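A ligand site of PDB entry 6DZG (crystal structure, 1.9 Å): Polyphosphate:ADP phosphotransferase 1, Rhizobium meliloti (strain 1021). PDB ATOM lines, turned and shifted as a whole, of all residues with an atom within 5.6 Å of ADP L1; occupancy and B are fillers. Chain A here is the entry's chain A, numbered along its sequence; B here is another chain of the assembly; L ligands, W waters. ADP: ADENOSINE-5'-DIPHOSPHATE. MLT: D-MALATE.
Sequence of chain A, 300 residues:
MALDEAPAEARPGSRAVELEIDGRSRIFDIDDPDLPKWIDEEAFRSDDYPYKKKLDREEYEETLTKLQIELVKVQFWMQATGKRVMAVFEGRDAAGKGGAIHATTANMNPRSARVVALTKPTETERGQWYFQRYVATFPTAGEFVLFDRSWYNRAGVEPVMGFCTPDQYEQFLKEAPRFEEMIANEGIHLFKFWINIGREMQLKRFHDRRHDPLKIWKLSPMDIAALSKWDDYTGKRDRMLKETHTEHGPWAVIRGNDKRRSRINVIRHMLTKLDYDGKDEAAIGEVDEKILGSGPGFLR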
ATOM      1  N   LYS A  97       1.832 -16.593   3.650  1.00  0.00           N
ATOM      2  CA  LYS A  97       1.180 -15.299   3.815  1.00  0.00           C
ATOM      3  C   LYS A  97       2.138 -14.147   3.565  1.00  0.00           C
ATOM      4  O   LYS A  97       1.722 -13.103   3.042  1.00  0.00           O
ATOM      5  CB  LYS A  97       0.518 -15.186   5.190  1.00  0.00           C
ATOM      6  CG  LYS A  97       1.283 -15.808   6.324  1.00  0.00           C
ATOM      7  CD  LYS A  97       0.447 -15.832   7.590  1.00  0.00           C
ATOM      8  CE  LYS A  97       1.174 -16.571   8.686  1.00  0.00           C
ATOM      9  NZ  LYS A  97       2.534 -15.997   8.954  1.00  0.00           N
ATOM     10  N   LEU A 118       3.517  -8.169  14.456  1.00  0.00           N
ATOM     11  CA  LEU A 118       3.810  -7.964  15.864  1.00  0.00           C
ATOM     12  C   LEU A 118       4.514  -9.195  16.439  1.00  0.00           C
ATOM     13  O   LEU A 118       4.340 -10.315  15.959  1.00  0.00           O
ATOM     14  CB  LEU A 118       2.531  -7.692  16.651  1.00  0.00           C
ATOM     15  CG  LEU A 118       1.623  -6.517  16.234  1.00  0.00           C
ATOM     16  CD1 LEU A 118       0.579  -6.289  17.318  1.00  0.00           C
ATOM     17  CD2 LEU A 118       2.444  -5.246  16.021  1.00  0.00           C
ATOM     18  N   THR A 119       5.314  -8.949  17.476  1.00  0.00           N
ATOM     19  CA  THR A 119       5.957  -9.986  18.260  1.00  0.00           C
ATOM     20  C   THR A 119       5.081 -10.329  19.459  1.00  0.00           C
ATOM     21  O   THR A 119       3.988  -9.793  19.638  1.00  0.00           O
ATOM     22  CB  THR A 119       7.349  -9.523  18.691  1.00  0.00           C
ATOM     23  OG1 THR A 119       7.222  -8.360  19.526  1.00  0.00           O
ATOM     24  CG2 THR A 119       8.194  -9.178  17.465  1.00  0.00           C
ATOM     25  N   LYS A 120       5.578 -11.230  20.306  1.00  0.00           N
ATOM     26  CA  LYS A 120       4.729 -11.722  21.372  1.00  0.00           C
ATOM     27  C   LYS A 120       4.479 -10.610  22.388  1.00  0.00           C
ATOM     28  O   LYS A 120       5.322  -9.736  22.595  1.00  0.00           O
ATOM     29  CB  LYS A 120       5.356 -12.944  22.057  1.00  0.00           C
ATOM     30  CG  LYS A 120       6.618 -12.646  22.837  1.00  0.00           C
ATOM     31  CD  LYS A 120       7.247 -13.924  23.359  1.00  0.00           C
ATOM     32  CE  LYS A 120       8.483 -13.593  24.167  1.00  0.00           C
ATOM     33  NZ  LYS A 120       9.238 -14.816  24.580  1.00  0.00           N
ATOM     34  N   PRO A 121       3.314 -10.619  23.021  1.00  0.00           N
ATOM     35  CA  PRO A 121       2.944  -9.476  23.869  1.00  0.00           C
ATOM     36  C   PRO A 121       3.830  -9.344  25.101  1.00  0.00           C
ATOM     37  O   PRO A 121       4.230 -10.337  25.723  1.00  0.00           O
ATOM     38  CB  PRO A 121       1.484  -9.782  24.257  1.00  0.00           C
ATOM     39  CG  PRO A 121       1.313 -11.240  23.997  1.00  0.00           C
ATOM     40  CD  PRO A 121       2.209 -11.571  22.841  1.00  0.00           C
ATOM     41  N   ASP A 148       0.477  -9.481   8.859  1.00  0.00           N
ATOM     42  CA  ASP A 148       1.164 -10.765   8.750  1.00  0.00           C
ATOM     43  C   ASP A 148       0.945 -11.475  10.087  1.00  0.00           C
ATOM     44  O   ASP A 148       1.767 -11.372  11.010  1.00  0.00           O
ATOM     45  CB  ASP A 148       2.630 -10.538   8.418  1.00  0.00           C
ATOM     46  CG  ASP A 148       3.466 -11.818   8.483  1.00  0.00           C
ATOM     47  OD1 ASP A 148       2.900 -12.931   8.614  1.00  0.00           O
ATOM     48  OD2 ASP A 148       4.708 -11.698   8.413  1.00  0.00           O
ATOM     49  N   ARG A 149      -0.169 -12.208  10.161  1.00  0.00           N
ATOM     50  CA  ARG A 149      -0.828 -12.669  11.401  1.00  0.00           C
ATOM     51  C   ARG A 149      -1.510 -11.470  12.072  1.00  0.00           C
ATOM     52  O   ARG A 149      -1.239 -10.314  11.738  1.00  0.00           O
ATOM     53  CB  ARG A 149       0.144 -13.348  12.367  1.00  0.00           C
ATOM     54  CG  ARG A 149       0.633 -14.723  11.921  1.00  0.00           C
ATOM     55  CD  ARG A 149       1.521 -15.315  12.974  1.00  0.00           C
ATOM     56  NE  ARG A 149       2.151 -16.526  12.487  1.00  0.00           N
ATOM     57  CZ  ARG A 149       1.660 -17.752  12.663  1.00  0.00           C
ATOM     58  NH1 ARG A 149       0.539 -17.931  13.340  1.00  0.00           N
ATOM     59  NH2 ARG A 149       2.324 -18.804  12.180  1.00  0.00           N
ATOM     60  N   ASN A 153      -4.300 -14.580  16.070  1.00  0.00           N
ATOM     61  CA  ASN A 153      -3.413 -15.423  16.887  1.00  0.00           C
ATOM     62  C   ASN A 153      -4.204 -16.171  17.961  1.00  0.00           C
ATOM     63  O   ASN A 153      -3.960 -17.353  18.207  1.00  0.00           O
ATOM     64  CB  ASN A 153      -2.334 -14.567  17.531  1.00  0.00           C
ATOM     65  CG  ASN A 153      -1.129 -14.373  16.644  1.00  0.00           C
ATOM     66  OD1 ASN A 153      -1.254 -14.307  15.444  1.00  0.00           O
ATOM     67  ND2 ASN A 153       0.054 -14.303  17.241  1.00  0.00           N
ATOM     68  N   VAL A 157      -2.619 -20.178  17.022  1.00  0.00           N
ATOM     69  CA  VAL A 157      -1.364 -20.537  17.666  1.00  0.00           C
ATOM     70  C   VAL A 157      -1.471 -20.432  19.188  1.00  0.00           C
ATOM     71  O   VAL A 157      -0.950 -21.289  19.910  1.00  0.00           O
ATOM     72  CB  VAL A 157      -0.201 -19.680  17.114  1.00  0.00           C
ATOM     73  CG1 VAL A 157      -0.479 -18.188  17.282  1.00  0.00           C
ATOM     74  CG2 VAL A 157       1.146 -20.135  17.771  1.00  0.00           C
ATOM     75  N   GLU A 158      -2.159 -19.408  19.716  1.00  0.00           N
ATOM     76  CA  GLU A 158      -2.211 -19.265  21.163  1.00  0.00           C
ATOM     77  C   GLU A 158      -2.945 -20.432  21.837  1.00  0.00           C
ATOM     78  O   GLU A 158      -2.338 -21.071  22.705  1.00  0.00           O
ATOM     79  CB  GLU A 158      -2.819 -17.907  21.561  1.00  0.00           C
ATOM     80  CG  GLU A 158      -1.986 -16.704  21.106  1.00  0.00           C
ATOM     81  CD  GLU A 158      -2.434 -15.390  21.787  1.00  0.00           C
ATOM     82  OE1 GLU A 158      -3.433 -15.401  22.524  1.00  0.00           O
ATOM     83  OE2 GLU A 158      -1.781 -14.347  21.586  1.00  0.00           O
ATOM     84  N   PHE A 163      -0.742 -20.604  24.973  1.00  0.00           N
ATOM     85  CA  PHE A 163      -0.347 -19.229  25.297  1.00  0.00           C
ATOM     86  C   PHE A 163      -1.522 -18.374  25.741  1.00  0.00           C
ATOM     87  O   PHE A 163      -1.316 -17.206  26.098  1.00  0.00           O
ATOM     88  CB  PHE A 163       0.290 -18.532  24.082  1.00  0.00           C
ATOM     89  CG  PHE A 163       1.497 -19.231  23.537  1.00  0.00           C
ATOM     90  CD1 PHE A 163       2.351 -19.940  24.353  1.00  0.00           C
ATOM     91  CD2 PHE A 163       1.788 -19.153  22.178  1.00  0.00           C
ATOM     92  CE1 PHE A 163       3.466 -20.577  23.827  1.00  0.00           C
ATOM     93  CE2 PHE A 163       2.891 -19.784  21.648  1.00  0.00           C
ATOM     94  CZ  PHE A 163       3.736 -20.501  22.486  1.00  0.00           C
ATOM     95  N   LYS A 218      12.692 -18.684   7.749  1.00  0.00           N
ATOM     96  CA  LYS A 218      11.250 -18.863   7.768  1.00  0.00           C
ATOM     97  C   LYS A 218      10.791 -19.933   8.750  1.00  0.00           C
ATOM     98  O   LYS A 218       9.582 -20.035   9.000  1.00  0.00           O
ATOM     99  CB  LYS A 218      10.746 -19.215   6.361  1.00  0.00           C
ATOM    100  CG  LYS A 218      10.864 -18.071   5.349  1.00  0.00           C
ATOM    101  CD  LYS A 218      10.317 -18.512   3.992  1.00  0.00           C
ATOM    102  CE  LYS A 218      10.311 -17.380   2.981  1.00  0.00           C
ATOM    103  NZ  LYS A 218       9.792 -17.872   1.674  1.00  0.00           N
ATOM    104  N   SER A 220      10.664 -21.688  12.584  1.00  0.00           N
ATOM    105  CA  SER A 220      10.704 -21.251  13.966  1.00  0.00           C
ATOM    106  C   SER A 220      10.290 -22.418  14.847  1.00  0.00           C
ATOM    107  O   SER A 220       9.728 -23.401  14.342  1.00  0.00           O
ATOM    108  CB  SER A 220       9.791 -20.046  14.193  1.00  0.00           C
ATOM    109  OG  SER A 220       8.454 -20.461  14.390  1.00  0.00           O
ATOM    110  N   MET A 222       7.828 -22.523  16.649  1.00  0.00           N
ATOM    111  CA  MET A 222       6.373 -22.611  16.492  1.00  0.00           C
ATOM    112  C   MET A 222       6.042 -23.547  15.353  1.00  0.00           C
ATOM    113  O   MET A 222       5.184 -24.419  15.491  1.00  0.00           O
ATOM    114  CB  MET A 222       5.760 -21.230  16.219  1.00  0.00           C
ATOM    115  CG  MET A 222       5.797 -20.297  17.411  1.00  0.00           C
ATOM    116  SD  MET A 222       5.119 -21.178  19.017  1.00  0.00           S
ATOM    117  CE  MET A 222       6.817 -21.680  19.866  1.00  0.00           C
ATOM    118  N   ASP A 223       6.726 -23.356  14.214  1.00  0.00           N
ATOM    119  CA  ASP A 223       6.580 -24.272  13.092  1.00  0.00           C
ATOM    120  C   ASP A 223       6.951 -25.691  13.490  1.00  0.00           C
ATOM    121  O   ASP A 223       6.206 -26.637  13.226  1.00  0.00           O
ATOM    122  CB  ASP A 223       7.437 -23.804  11.918  1.00  0.00           C
ATOM    123  CG  ASP A 223       7.041 -22.414  11.429  1.00  0.00           C
ATOM    124  OD1 ASP A 223       5.836 -22.102  11.407  1.00  0.00           O
ATOM    125  OD2 ASP A 223       7.952 -21.638  11.085  1.00  0.00           O
ATOM    126  N   ASN B 109      13.331 -11.738   8.480  1.00  0.00           N
ATOM    127  CA  ASN B 109      12.119 -11.950   9.256  1.00  0.00           C
ATOM    128  C   ASN B 109      11.441 -10.606   9.497  1.00  0.00           C
ATOM    129  O   ASN B 109      11.992  -9.766  10.218  1.00  0.00           O
ATOM    130  CB  ASN B 109      12.477 -12.615  10.580  1.00  0.00           C
ATOM    131  CG  ASN B 109      11.265 -13.169  11.313  1.00  0.00           C
ATOM    132  OD1 ASN B 109      10.157 -12.629  11.225  1.00  0.00           O
ATOM    133  ND2 ASN B 109      11.473 -14.267  12.035  1.00  0.00           N
ATOM    134  N   PRO B 110      10.232 -10.381   8.972  1.00  0.00           N
ATOM    135  CA  PRO B 110       9.591  -9.069   9.176  1.00  0.00           C
ATOM    136  C   PRO B 110       9.279  -8.767  10.648  1.00  0.00           C
ATOM    137  O   PRO B 110       8.955  -7.615  10.954  1.00  0.00           O
ATOM    138  CB  PRO B 110       8.310  -9.176   8.350  1.00  0.00           C
ATOM    139  CG  PRO B 110       8.036 -10.647   8.234  1.00  0.00           C
ATOM    140  CD  PRO B 110       9.394 -11.299   8.177  1.00  0.00           C
ATOM    141  N   ARG B 111       9.386  -9.728  11.555  1.00  0.00           N
ATOM    142  CA  ARG B 111       9.154  -9.428  12.968  1.00  0.00           C
ATOM    143  C   ARG B 111      10.394  -8.899  13.658  1.00  0.00           C
ATOM    144  O   ARG B 111      10.284  -8.424  14.792  1.00  0.00           O
ATOM    145  CB  ARG B 111       8.627 -10.663  13.709  1.00  0.00           C
ATOM    146  CG  ARG B 111       7.258 -11.115  13.184  1.00  0.00           C
ATOM    147  CD  ARG B 111       6.573 -12.210  13.984  1.00  0.00           C
ATOM    148  NE  ARG B 111       5.663 -12.904  13.072  1.00  0.00           N
ATOM    149  CZ  ARG B 111       4.469 -12.448  12.707  1.00  0.00           C
ATOM    150  NH1 ARG B 111       4.007 -11.316  13.236  1.00  0.00           N
ATOM    151  NH2 ARG B 111       3.744 -13.122  11.813  1.00  0.00           N
HETATM  152  PB  ADP L   1       6.520 -15.900  11.920  1.00  0.00           P
HETATM  153  O1B ADP L   1       7.192 -17.149  11.378  1.00  0.00           O
HETATM  154  O2B ADP L   1       5.148 -15.839  11.421  1.00  0.00           O
HETATM  155  O3B ADP L   1       7.264 -14.709  11.431  1.00  0.00           O
HETATM  156  PA  ADP L   1       6.844 -17.210  14.502  1.00  0.00           P
HETATM  157  O1A ADP L   1       6.831 -18.488  13.716  1.00  0.00           O
HETATM  158  O2A ADP L   1       8.190 -17.004  15.218  1.00  0.00           O
HETATM  159  O3A ADP L   1       6.518 -15.908  13.524  1.00  0.00           O
HETATM  160  O5' ADP L   1       5.635 -17.340  15.677  1.00  0.00           O
HETATM  161  C5' ADP L   1       4.300 -17.533  15.181  1.00  0.00           C
HETATM  162  C4' ADP L   1       3.345 -16.651  16.016  1.00  0.00           C
HETATM  163  O4' ADP L   1       3.317 -17.117  17.394  1.00  0.00           O
HETATM  164  C3' ADP L   1       3.905 -15.215  16.110  1.00  0.00           C
HETATM  165  O3' ADP L   1       2.823 -14.293  15.931  1.00  0.00           O
HETATM  166  C2' ADP L   1       4.402 -15.204  17.578  1.00  0.00           C
HETATM  167  O2' ADP L   1       4.386 -13.810  18.116  1.00  0.00           O
HETATM  168  C1' ADP L   1       3.600 -16.011  18.235  1.00  0.00           C
HETATM  169  N9  ADP L   1       4.225 -16.438  19.468  1.00  0.00           N
HETATM  170  C8  ADP L   1       5.422 -17.043  19.591  1.00  0.00           C
HETATM  171  N7  ADP L   1       5.690 -17.267  20.892  1.00  0.00           N
HETATM  172  C5  ADP L   1       4.648 -16.817  21.610  1.00  0.00           C
HETATM  173  C6  ADP L   1       4.394 -16.774  22.953  1.00  0.00           C
HETATM  174  N6  ADP L   1       5.375 -17.331  23.877  1.00  0.00           N
HETATM  175  N1  ADP L   1       3.261 -16.239  23.399  1.00  0.00           N
HETATM  176  C2  ADP L   1       2.349 -15.727  22.532  1.00  0.00           C
HETATM  177  N3  ADP L   1       2.575 -15.757  21.191  1.00  0.00           N
HETATM  178  C4  ADP L   1       3.719 -16.287  20.714  1.00  0.00           C
HETATM  179  C1  MLT L   2       4.562 -18.081   5.456  1.00  0.00           C
HETATM  180  O1  MLT L   2       4.862 -19.121   4.851  1.00  0.00           O
HETATM  181  O2  MLT L   2       3.369 -17.938   5.778  1.00  0.00           O
HETATM  182  C2  MLT L   2       5.602 -17.017   5.772  1.00  0.00           C
HETATM  183  O3  MLT L   2       5.026 -15.736   5.849  1.00  0.00           O
HETATM  184  C3  MLT L   2       6.763 -16.989   4.775  1.00  0.00           C
HETATM  185  C4  MLT L   2       6.342 -16.636   3.368  1.00  0.00           C
HETATM  186  O4  MLT L   2       7.170 -16.594   2.422  1.00  0.00           O
HETATM  187  O5  MLT L   2       5.146 -16.387   3.123  1.00  0.00           O
HETATM  188  O   HOH W   1       0.285 -14.428  20.036  1.00  0.00           O
HETATM  189  O   HOH W   2       2.136 -12.565  19.141  1.00  0.00           O
HETATM  190  O   HOH W   3       2.094 -11.594  16.504  1.00  0.00           O
HETATM  191  O   HOH W   4       6.998 -13.276  17.549  1.00  0.00           O
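The side-chain hydroxyl of Ser 220 sits at hydrogen-bond distance from an oxygen (O1A) of ADP L1 (2.6 Å).
NE of Arg 111 of chain B lies within salt-bridge range of O3B of ADP L1 (2.9 Å).
An oxygen (O3') of ADP L1 lies within hydrogen-bond range of the side-chain amide nitrogen of Asn 153 (3.1 Å).
O2B of ADP L1 is in salt-bridge range of NE of Arg 149, at 3.3 Å.
NZ of Lys 97 is in salt-bridge range of O2B of ADP L1, at 3.6 Å.
The backbone NH (N) of Lys 97 is in hydrogen-bond range of an oxygen (O2) of MLT L2 (2.9 Å).
An oxygen (O2) of MLT L2 is in salt-bridge range of the side-chain amino group of Lys 97 (3.8 Å).
The side-chain amino group (NZ) of Lys 218 is in salt-bridge range of an oxygen (O4) of MLT L2 (3.0 Å).
The side-chain hydroxyl (OG) of Ser 220 sits close to the backbone NH (N) of Met 222, at 3.1 Å.
The backbone NH of Ser 220 lies within hydrogen-bond range of the side-chain carboxylate of Asp 223 (3.1 Å).
OD1 of Asn 109 of chain B lies within hydrogen-bond range of N of Arg 111 of chain B, at 3.0 Å.
The backbone carbonyl oxygen (O) of Leu 118 is in hydrogen-bond range of the guanidinium group (NH1) of Arg 111 of chain B (2.9 Å).
The guanidinium group (NH2) of Arg 111 of chain B is in salt-bridge range of the side-chain carboxylate (OD1) of Asp 148 (3.3 Å).
The backbone NH (N) of Glu 158 sits at hydrogen-bond distance from the backbone carbonyl oxygen (O) of Asn 153.
The backbone carbonyl oxygen (O) of Glu 158 is in hydrogen-bond range of the backbone NH (N) of Phe 163 (2.8 Å).
The side-chain amino group (NZ) of Lys 97 lies within salt-bridge range of the side-chain carboxylate (OD1) of Asp 148 (3.1 Å).
Thr 119 touches ADP L1.
Lys 120 touches ADP L1 (N to O2', 3.6 Å).
Val 157 touches ADP L1.
CE2 of Phe 163 touches C5 of ADP L1 (3.4 Å).
Met 222 touches ADP L1 (CG to O5', 3.4 Å).
Asn 109 of chain B touches ADP L1.
Hydrophobic or aromatic side chains within 4 Å of ADP L1: Val 157, Phe 163 and Met 222.
Of the 18 residues printed, 11 come within 4 Å of ADP L1.
Water W2 lies within hydrogen-bond range of O2' of ADP L1 (2.8 Å), ND2 of Asn 153 (3.3 Å) and O of Thr 119 (3.4 Å).
Water W3 lies within hydrogen-bond range of O of Leu 118 (2.6 Å), O3' of ADP L1 (2.9 Å) and ND2 of Asn 153 (3.5 Å).
Water W1 lies within hydrogen-bond range of the side-chain carboxylate (OE2) of Glu 158, the side-chain amide nitrogen (ND2) of Asn 153 and a nitrogen (N3) of ADP L1.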
